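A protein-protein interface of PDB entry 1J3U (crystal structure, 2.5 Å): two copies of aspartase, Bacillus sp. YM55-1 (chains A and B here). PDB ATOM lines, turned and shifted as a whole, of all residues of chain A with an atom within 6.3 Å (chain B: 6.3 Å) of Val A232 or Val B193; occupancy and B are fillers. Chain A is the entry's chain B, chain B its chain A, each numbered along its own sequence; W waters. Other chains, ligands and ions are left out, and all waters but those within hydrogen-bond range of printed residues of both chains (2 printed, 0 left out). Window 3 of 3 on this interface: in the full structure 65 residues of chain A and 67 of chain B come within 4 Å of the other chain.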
ATOM      1  N   SER A 140     -26.795  34.751  15.637  1.00  0.00           N
ATOM      2  CA  SER A 140     -25.728  34.218  16.473  1.00  0.00           C
ATOM      3  C   SER A 140     -24.715  33.497  15.589  1.00  0.00           C
ATOM      4  O   SER A 140     -25.014  33.121  14.457  1.00  0.00           O
ATOM      5  CB  SER A 140     -26.301  33.238  17.505  1.00  0.00           C
ATOM      6  OG  SER A 140     -25.278  32.716  18.337  1.00  0.00           O
ATOM      7  N   ASN A 142     -23.952  30.701  15.676  1.00  0.00           N
ATOM      8  CA  ASN A 142     -24.419  29.334  15.449  1.00  0.00           C
ATOM      9  C   ASN A 142     -25.522  29.195  14.400  1.00  0.00           C
ATOM     10  O   ASN A 142     -26.022  28.096  14.174  1.00  0.00           O
ATOM     11  CB  ASN A 142     -24.890  28.696  16.769  1.00  0.00           C
ATOM     12  CG  ASN A 142     -23.767  28.553  17.794  1.00  0.00           C
ATOM     13  OD1 ASN A 142     -22.613  28.321  17.440  1.00  0.00           O
ATOM     14  ND2 ASN A 142     -24.111  28.674  19.070  1.00  0.00           N
ATOM     15  N   ALA A 229     -32.458  30.663  14.794  1.00  0.00           N
ATOM     16  CA  ALA A 229     -32.184  29.874  15.982  1.00  0.00           C
ATOM     17  C   ALA A 229     -31.279  30.819  16.739  1.00  0.00           C
ATOM     18  O   ALA A 229     -30.438  31.485  16.137  1.00  0.00           O
ATOM     19  CB  ALA A 229     -31.433  28.604  15.617  1.00  0.00           C
ATOM     20  N   THR A 230     -31.455  30.925  18.043  1.00  0.00           N
ATOM     21  CA  THR A 230     -30.592  31.823  18.784  1.00  0.00           C
ATOM     22  C   THR A 230     -29.227  31.168  18.952  1.00  0.00           C
ATOM     23  O   THR A 230     -28.540  30.888  17.971  1.00  0.00           O
ATOM     24  CB  THR A 230     -31.196  32.159  20.150  1.00  0.00           C
ATOM     25  OG1 THR A 230     -31.915  31.019  20.642  1.00  0.00           O
ATOM     26  CG2 THR A 230     -32.127  33.359  20.033  1.00  0.00           C
ATOM     27  N   ALA A 231     -28.836  30.919  20.195  1.00  0.00           N
ATOM     28  CA  ALA A 231     -27.555  30.293  20.470  1.00  0.00           C
ATOM     29  C   ALA A 231     -27.709  28.789  20.360  1.00  0.00           C
ATOM     30  O   ALA A 231     -27.050  28.141  19.556  1.00  0.00           O
ATOM     31  CB  ALA A 231     -27.076  30.668  21.869  1.00  0.00           C
ATOM     32  N   VAL A 232     -28.605  28.249  21.174  1.00  0.00           N
ATOM     33  CA  VAL A 232     -28.858  26.823  21.214  1.00  0.00           C
ATOM     34  C   VAL A 232     -29.842  26.359  20.145  1.00  0.00           C
ATOM     35  O   VAL A 232     -29.954  25.164  19.871  1.00  0.00           O
ATOM     36  CB  VAL A 232     -29.375  26.431  22.610  1.00  0.00           C
ATOM     37  CG1 VAL A 232     -29.857  24.993  22.619  1.00  0.00           C
ATOM     38  CG2 VAL A 232     -28.268  26.612  23.626  1.00  0.00           C
ATOM     39  N   GLY A 233     -30.552  27.301  19.537  1.00  0.00           N
ATOM     40  CA  GLY A 233     -31.513  26.941  18.509  1.00  0.00           C
ATOM     41  C   GLY A 233     -32.938  26.950  19.020  1.00  0.00           C
ATOM     42  O   GLY A 233     -33.843  26.449  18.359  1.00  0.00           O
ATOM     43  N   THR A 234     -33.132  27.525  20.204  1.00  0.00           N
ATOM     44  CA  THR A 234     -34.448  27.616  20.817  1.00  0.00           C
ATOM     45  C   THR A 234     -35.141  28.908  20.417  1.00  0.00           C
ATOM     46  O   THR A 234     -36.286  29.142  20.784  1.00  0.00           O
ATOM     47  CB  THR A 234     -34.342  27.578  22.330  1.00  0.00           C
ATOM     48  OG1 THR A 234     -33.372  28.539  22.751  1.00  0.00           O
ATOM     49  CG2 THR A 234     -33.934  26.200  22.802  1.00  0.00           C
ATOM     50  N   GLY A 235     -34.434  29.749  19.671  1.00  0.00           N
ATOM     51  CA  GLY A 235     -35.002  31.006  19.207  1.00  0.00           C
ATOM     52  C   GLY A 235     -35.391  31.981  20.301  1.00  0.00           C
ATOM     53  O   GLY A 235     -36.238  32.848  20.090  1.00  0.00           O
ATOM     54  N   LEU A 236     -34.764  31.842  21.466  1.00  0.00           N
ATOM     55  CA  LEU A 236     -35.037  32.706  22.610  1.00  0.00           C
ATOM     56  C   LEU A 236     -34.933  34.183  22.238  1.00  0.00           C
ATOM     57  O   LEU A 236     -33.876  34.655  21.812  1.00  0.00           O
ATOM     58  CB  LEU A 236     -34.063  32.381  23.750  1.00  0.00           C
ATOM     59  CG  LEU A 236     -34.276  33.050  25.112  1.00  0.00           C
ATOM     60  CD1 LEU A 236     -35.655  32.721  25.658  1.00  0.00           C
ATOM     61  CD2 LEU A 236     -33.202  32.571  26.070  1.00  0.00           C
ATOM     62  N   LEU A 264     -35.554  23.844  14.965  1.00  0.00           N
ATOM     63  CA  LEU A 264     -34.300  24.571  15.008  1.00  0.00           C
ATOM     64  C   LEU A 264     -33.225  23.962  15.902  1.00  0.00           C
ATOM     65  O   LEU A 264     -32.045  24.061  15.589  1.00  0.00           O
ATOM     66  CB  LEU A 264     -34.557  26.036  15.385  1.00  0.00           C
ATOM     67  CG  LEU A 264     -34.716  26.997  14.190  1.00  0.00           C
ATOM     68  CD1 LEU A 264     -35.826  26.518  13.260  1.00  0.00           C
ATOM     69  CD2 LEU A 264     -35.014  28.392  14.687  1.00  0.00           C
ATOM     70  N   VAL A 265     -33.612  23.336  17.009  1.00  0.00           N
ATOM     71  CA  VAL A 265     -32.619  22.729  17.892  1.00  0.00           C
ATOM     72  C   VAL A 265     -31.939  21.595  17.116  1.00  0.00           C
ATOM     73  O   VAL A 265     -30.728  21.375  17.222  1.00  0.00           O
ATOM     74  CB  VAL A 265     -33.272  22.185  19.188  1.00  0.00           C
ATOM     75  CG1 VAL A 265     -32.254  21.475  20.032  1.00  0.00           C
ATOM     76  CG2 VAL A 265     -33.854  23.326  19.982  1.00  0.00           C
ATOM     77  N   ASP A 266     -32.728  20.885  16.320  1.00  0.00           N
ATOM     78  CA  ASP A 266     -32.205  19.796  15.513  1.00  0.00           C
ATOM     79  C   ASP A 266     -31.248  20.355  14.455  1.00  0.00           C
ATOM     80  O   ASP A 266     -30.095  19.913  14.352  1.00  0.00           O
ATOM     81  CB  ASP A 266     -33.369  19.025  14.863  1.00  0.00           C
ATOM     82  CG  ASP A 266     -33.030  18.495  13.480  1.00  0.00           C
ATOM     83  OD1 ASP A 266     -32.000  17.813  13.334  1.00  0.00           O
ATOM     84  OD2 ASP A 266     -33.808  18.760  12.540  1.00  0.00           O
ATOM     85  N   THR A 268     -29.609  22.826  14.481  1.00  0.00           N
ATOM     86  CA  THR A 268     -28.482  23.530  15.065  1.00  0.00           C
ATOM     87  C   THR A 268     -27.368  22.600  15.508  1.00  0.00           C
ATOM     88  O   THR A 268     -26.196  22.892  15.283  1.00  0.00           O
ATOM     89  CB  THR A 268     -28.908  24.389  16.284  1.00  0.00           C
ATOM     90  OG1 THR A 268     -29.836  25.398  15.866  1.00  0.00           O
ATOM     91  CG2 THR A 268     -27.689  25.060  16.913  1.00  0.00           C
ATOM     92  N   GLN A 269     -27.725  21.485  16.131  1.00  0.00           N
ATOM     93  CA  GLN A 269     -26.718  20.564  16.617  1.00  0.00           C
ATOM     94  C   GLN A 269     -26.330  19.422  15.676  1.00  0.00           C
ATOM     95  O   GLN A 269     -25.247  18.837  15.828  1.00  0.00           O
ATOM     96  CB  GLN A 269     -27.141  19.994  17.968  1.00  0.00           C
ATOM     97  CG  GLN A 269     -28.528  19.406  18.003  1.00  0.00           C
ATOM     98  CD  GLN A 269     -28.844  18.794  19.347  1.00  0.00           C
ATOM     99  OE1 GLN A 269     -28.640  17.592  19.574  1.00  0.00           O
ATOM    100  NE2 GLN A 269     -29.329  19.624  20.263  1.00  0.00           N
ATOM    101  N   GLU A 357     -25.985  20.798  22.048  1.00  0.00           N
ATOM    102  CA  GLU A 357     -26.575  21.699  21.056  1.00  0.00           C
ATOM    103  C   GLU A 357     -25.638  22.380  20.048  1.00  0.00           C
ATOM    104  O   GLU A 357     -26.085  23.215  19.258  1.00  0.00           O
ATOM    105  CB  GLU A 357     -27.448  22.763  21.740  1.00  0.00           C
ATOM    106  CG  GLU A 357     -27.419  22.774  23.254  1.00  0.00           C
ATOM    107  CD  GLU A 357     -27.871  21.470  23.856  1.00  0.00           C
ATOM    108  OE1 GLU A 357     -28.735  20.803  23.245  1.00  0.00           O
ATOM    109  OE2 GLU A 357     -27.371  21.114  24.947  1.00  0.00           O
ATOM    110  N   LYS B 183     -33.824  21.836  31.170  1.00  0.00           N
ATOM    111  CA  LYS B 183     -32.433  21.571  31.512  1.00  0.00           C
ATOM    112  C   LYS B 183     -31.613  22.705  30.932  1.00  0.00           C
ATOM    113  O   LYS B 183     -32.154  23.592  30.281  1.00  0.00           O
ATOM    114  CB  LYS B 183     -31.960  20.241  30.924  1.00  0.00           C
ATOM    115  CG  LYS B 183     -32.174  20.132  29.435  1.00  0.00           C
ATOM    116  CD  LYS B 183     -31.338  19.027  28.813  1.00  0.00           C
ATOM    117  CE  LYS B 183     -29.865  19.366  28.864  1.00  0.00           C
ATOM    118  NZ  LYS B 183     -29.046  18.374  28.124  1.00  0.00           N
ATOM    119  N   MET B 184     -30.305  22.673  31.157  1.00  0.00           N
ATOM    120  CA  MET B 184     -29.422  23.733  30.674  1.00  0.00           C
ATOM    121  C   MET B 184     -28.652  23.347  29.413  1.00  0.00           C
ATOM    122  O   MET B 184     -27.859  22.404  29.422  1.00  0.00           O
ATOM    123  CB  MET B 184     -28.440  24.122  31.786  1.00  0.00           C
ATOM    124  CG  MET B 184     -27.619  25.376  31.521  1.00  0.00           C
ATOM    125  SD  MET B 184     -28.620  26.842  31.139  1.00  0.00           S
ATOM    126  CE  MET B 184     -29.923  26.658  32.316  1.00  0.00           C
ATOM    127  N   GLY B 185     -28.887  24.084  28.328  1.00  0.00           N
ATOM    128  CA  GLY B 185     -28.195  23.805  27.081  1.00  0.00           C
ATOM    129  C   GLY B 185     -26.717  24.119  27.188  1.00  0.00           C
ATOM    130  O   GLY B 185     -26.309  24.893  28.054  1.00  0.00           O
ATOM    131  N   ARG B 186     -25.911  23.520  26.312  1.00  0.00           N
ATOM    132  CA  ARG B 186     -24.463  23.749  26.321  1.00  0.00           C
ATOM    133  C   ARG B 186     -23.906  23.800  24.906  1.00  0.00           C
ATOM    134  O   ARG B 186     -24.314  23.018  24.057  1.00  0.00           O
ATOM    135  CB  ARG B 186     -23.741  22.624  27.085  1.00  0.00           C
ATOM    136  CG  ARG B 186     -24.237  22.382  28.512  1.00  0.00           C
ATOM    137  CD  ARG B 186     -23.453  21.266  29.200  1.00  0.00           C
ATOM    138  NE  ARG B 186     -23.963  20.930  30.537  1.00  0.00           N
ATOM    139  CZ  ARG B 186     -24.971  20.093  30.778  1.00  0.00           C
ATOM    140  NH1 ARG B 186     -25.605  19.490  29.780  1.00  0.00           N
ATOM    141  NH2 ARG B 186     -25.347  19.854  32.023  1.00  0.00           N
ATOM    142  N   THR B 187     -22.988  24.733  24.657  1.00  0.00           N
ATOM    143  CA  THR B 187     -22.318  24.866  23.357  1.00  0.00           C
ATOM    144  C   THR B 187     -20.860  25.074  23.718  1.00  0.00           C
ATOM    145  O   THR B 187     -20.550  25.996  24.480  1.00  0.00           O
ATOM    146  CB  THR B 187     -22.779  26.090  22.561  1.00  0.00           C
ATOM    147  OG1 THR B 187     -22.436  27.273  23.280  1.00  0.00           O
ATOM    148  CG2 THR B 187     -24.271  26.039  22.315  1.00  0.00           C
ATOM    149  N   ASP B 191     -21.777  26.495  29.493  1.00  0.00           N
ATOM    150  CA  ASP B 191     -23.170  26.850  29.802  1.00  0.00           C
ATOM    151  C   ASP B 191     -23.680  27.776  28.719  1.00  0.00           C
ATOM    152  O   ASP B 191     -22.936  28.628  28.233  1.00  0.00           O
ATOM    153  CB  ASP B 191     -23.278  27.589  31.139  1.00  0.00           C
ATOM    154  CG  ASP B 191     -23.050  26.692  32.334  1.00  0.00           C
ATOM    155  OD1 ASP B 191     -23.054  27.215  33.464  1.00  0.00           O
ATOM    156  OD2 ASP B 191     -22.874  25.475  32.159  1.00  0.00           O
ATOM    157  N   ALA B 192     -24.939  27.616  28.344  1.00  0.00           N
ATOM    158  CA  ALA B 192     -25.523  28.457  27.314  1.00  0.00           C
ATOM    159  C   ALA B 192     -26.870  28.965  27.816  1.00  0.00           C
ATOM    160  O   ALA B 192     -26.971  29.477  28.929  1.00  0.00           O
ATOM    161  CB  ALA B 192     -25.693  27.656  26.041  1.00  0.00           C
ATOM    162  N   VAL B 193     -27.903  28.830  26.995  1.00  0.00           N
ATOM    163  CA  VAL B 193     -29.235  29.247  27.398  1.00  0.00           C
ATOM    164  C   VAL B 193     -30.029  27.977  27.670  1.00  0.00           C
ATOM    165  O   VAL B 193     -29.588  26.882  27.329  1.00  0.00           O
ATOM    166  CB  VAL B 193     -29.920  30.083  26.296  1.00  0.00           C
ATOM    167  CG1 VAL B 193     -29.267  31.454  26.208  1.00  0.00           C
ATOM    168  CG2 VAL B 193     -29.825  29.363  24.954  1.00  0.00           C
ATOM    169  N   PRO B 194     -31.200  28.100  28.306  1.00  0.00           N
ATOM    170  CA  PRO B 194     -32.030  26.928  28.611  1.00  0.00           C
ATOM    171  C   PRO B 194     -32.584  26.235  27.366  1.00  0.00           C
ATOM    172  O   PRO B 194     -32.742  26.860  26.312  1.00  0.00           O
ATOM    173  CB  PRO B 194     -33.139  27.508  29.486  1.00  0.00           C
ATOM    174  CG  PRO B 194     -32.480  28.679  30.130  1.00  0.00           C
ATOM    175  CD  PRO B 194     -31.718  29.293  28.985  1.00  0.00           C
ATOM    176  N   ILE B 195     -32.874  24.942  27.501  1.00  0.00           N
ATOM    177  CA  ILE B 195     -33.401  24.139  26.405  1.00  0.00           C
ATOM    178  C   ILE B 195     -34.184  22.975  26.992  1.00  0.00           C
ATOM    179  O   ILE B 195     -33.899  22.530  28.096  1.00  0.00           O
ATOM    180  CB  ILE B 195     -32.255  23.590  25.520  1.00  0.00           C
ATOM    181  CG1 ILE B 195     -32.829  22.805  24.341  1.00  0.00           C
ATOM    182  CG2 ILE B 195     -31.343  22.699  26.341  1.00  0.00           C
ATOM    183  CD1 ILE B 195     -31.779  22.295  23.368  1.00  0.00           C
ATOM    184  N   GLY B 407     -26.697  32.098  32.962  1.00  0.00           N
ATOM    185  CA  GLY B 407     -27.128  32.215  31.573  1.00  0.00           C
ATOM    186  C   GLY B 407     -28.618  32.382  31.337  1.00  0.00           C
ATOM    187  O   GLY B 407     -29.036  32.819  30.268  1.00  0.00           O
ATOM    188  N   ILE B 408     -29.420  32.022  32.329  1.00  0.00           N
ATOM    189  CA  ILE B 408     -30.870  32.156  32.227  1.00  0.00           C
ATOM    190  C   ILE B 408     -31.231  33.635  32.106  1.00  0.00           C
ATOM    191  O   ILE B 408     -32.356  33.985  31.756  1.00  0.00           O
ATOM    192  CB  ILE B 408     -31.564  31.585  33.478  1.00  0.00           C
ATOM    193  CG1 ILE B 408     -33.071  31.840  33.412  1.00  0.00           C
ATOM    194  CG2 ILE B 408     -30.972  32.214  34.722  1.00  0.00           C
ATOM    195  CD1 ILE B 408     -33.827  31.393  34.645  1.00  0.00           C
ATOM    196  N   THR B 410     -30.507  35.661  29.904  1.00  0.00           N
ATOM    197  CA  THR B 410     -30.842  36.047  28.538  1.00  0.00           C
ATOM    198  C   THR B 410     -32.355  35.977  28.341  1.00  0.00           C
ATOM    199  O   THR B 410     -32.917  36.714  27.533  1.00  0.00           O
ATOM    200  CB  THR B 410     -30.145  35.123  27.495  1.00  0.00           C
ATOM    201  OG1 THR B 410     -28.732  35.377  27.484  1.00  0.00           O
ATOM    202  CG2 THR B 410     -30.708  35.365  26.100  1.00  0.00           C
ATOM    203  N   ALA B 411     -33.009  35.099  29.097  1.00  0.00           N
ATOM    204  CA  ALA B 411     -34.458  34.927  29.007  1.00  0.00           C
ATOM    205  C   ALA B 411     -35.238  35.958  29.830  1.00  0.00           C
ATOM    206  O   ALA B 411     -36.461  36.054  29.723  1.00  0.00           O
ATOM    207  CB  ALA B 411     -34.836  33.518  29.449  1.00  0.00           C
ATOM    208  N   MET B 459     -39.575  29.864  27.222  1.00  0.00           N
ATOM    209  CA  MET B 459     -38.178  30.189  27.476  1.00  0.00           C
ATOM    210  C   MET B 459     -37.285  29.437  26.490  1.00  0.00           C
ATOM    211  O   MET B 459     -36.172  29.857  26.192  1.00  0.00           O
ATOM    212  CB  MET B 459     -37.827  29.807  28.917  1.00  0.00           C
ATOM    213  CG  MET B 459     -36.438  30.193  29.372  1.00  0.00           C
ATOM    214  SD  MET B 459     -36.295  30.047  31.157  1.00  0.00           S
ATOM    215  CE  MET B 459     -36.673  28.331  31.398  1.00  0.00           C
HETATM  216  O   HOH W   1     -33.812  29.225  25.627  1.00  0.00           O
HETATM  217  O   HOH W   2     -27.283  20.038  27.487  1.00  0.00           O
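Of the 15 printed residues of chain B, 9 touch a printed residue of chain A.
Hydrophobic or aromatic side chains of chain B that line the printed part of chain A: Ala B192, Val B193, Ile B195 and Ala B411.
Of the 16 printed residues of chain A, 5 touch a printed residue of chain B.
Hydrophobic or aromatic side chains of chain A that line the printed part of chain B: Val A232, Leu A236 and Val A265.
Among the printed residues, 12 pairs touch across the chains.
Among the printed residues, no Asp or Glu carboxylate lies within 4 Å of a Lys or Arg side-chain nitrogen of the other chain.
Water W2 lies within hydrogen-bond range of the side-chain amino group of Lys B183, the side-chain carboxylate of Glu A357, the guanidinium group of Arg B186 and the backbone carbonyl oxygen of Met B184.
Water W1 lies within hydrogen-bond range of the backbone carbonyl oxygen of Met B459 (2.5 Å), the backbone carbonyl oxygen of Pro B194 (2.7 Å) and the side-chain hydroxyl of Thr A234 (3.0 Å).
Among the printed residues, merely in contact across the chains: Leu A236 with Met B459, Glu A357 with Ile B195, Val A232 with Ile B195, Val A232 with Val B193, Val A265 with Ile B195, Glu A357 with Gly B185, Val A232 with Ala B192, Leu A236 with Thr B410, Thr A234 with Pro B194, Leu A236 with Ala B411 and Thr A234 with Ile B195.
Of chain B, only Ala B192, Val B193 and Ile B195 come within 4 Å of Val A232.
Of the printed residues of chain A, Val B193 touches Val A232 (3.4 Å).
Of the printed residues of chain A, Ala B411 touches Leu A236.
Printed residues of chain A within 4 Å of Met B459: Leu A236.
Printed residues of chain B within 4 Å of Glu A357: Gly B185 (3.5 Å), Arg B186 (3.1 Å) and Ile B195 (3.4 Å).
Of the printed residues of chain B, Val A265 touches Ile B195 (3.5 Å).
Asp B191 touches none of the printed residues of chain A.
Asp A266 touches none of the printed residues of chain B.
The nearest residue of chain A that does not touch Val B193 is Leu A236 (4.1 Å).
The nearest printed residue of chain A that does not touch Gly B185 is Val A232 (4.5 Å).
No position is printed for both chains.
The side-chain carboxylate of Glu A357 is in hydrogen-bond range of the backbone NH of Arg B186 (3.1 Å).
N of Val A265 is in hydrogen-bond range of O of Gly A233 (3.4 Å).
The side-chain hydroxyl (OG1) of Thr A230 sits at hydrogen-bond distance from the backbone NH (N) of Leu A236, at 3.1 Å.
The backbone NH (N) of Gly B185 is in hydrogen-bond range of the backbone carbonyl oxygen (O) of Val B193, at 3.1 Å.
The side-chain amide nitrogen (NE2) of Gln A269 lies within hydrogen-bond range of the side-chain carboxylate (OE1) of Glu A357 (3.3 Å).
The backbone NH (N) of Ala B192 is in hydrogen-bond range of the backbone carbonyl oxygen (O) of Gly B185, at 3.1 Å.
The backbone carbonyl oxygen (O) of Ile B195 sits at hydrogen-bond distance from the backbone NH (N) of Lys B183, 3.2 Å away.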
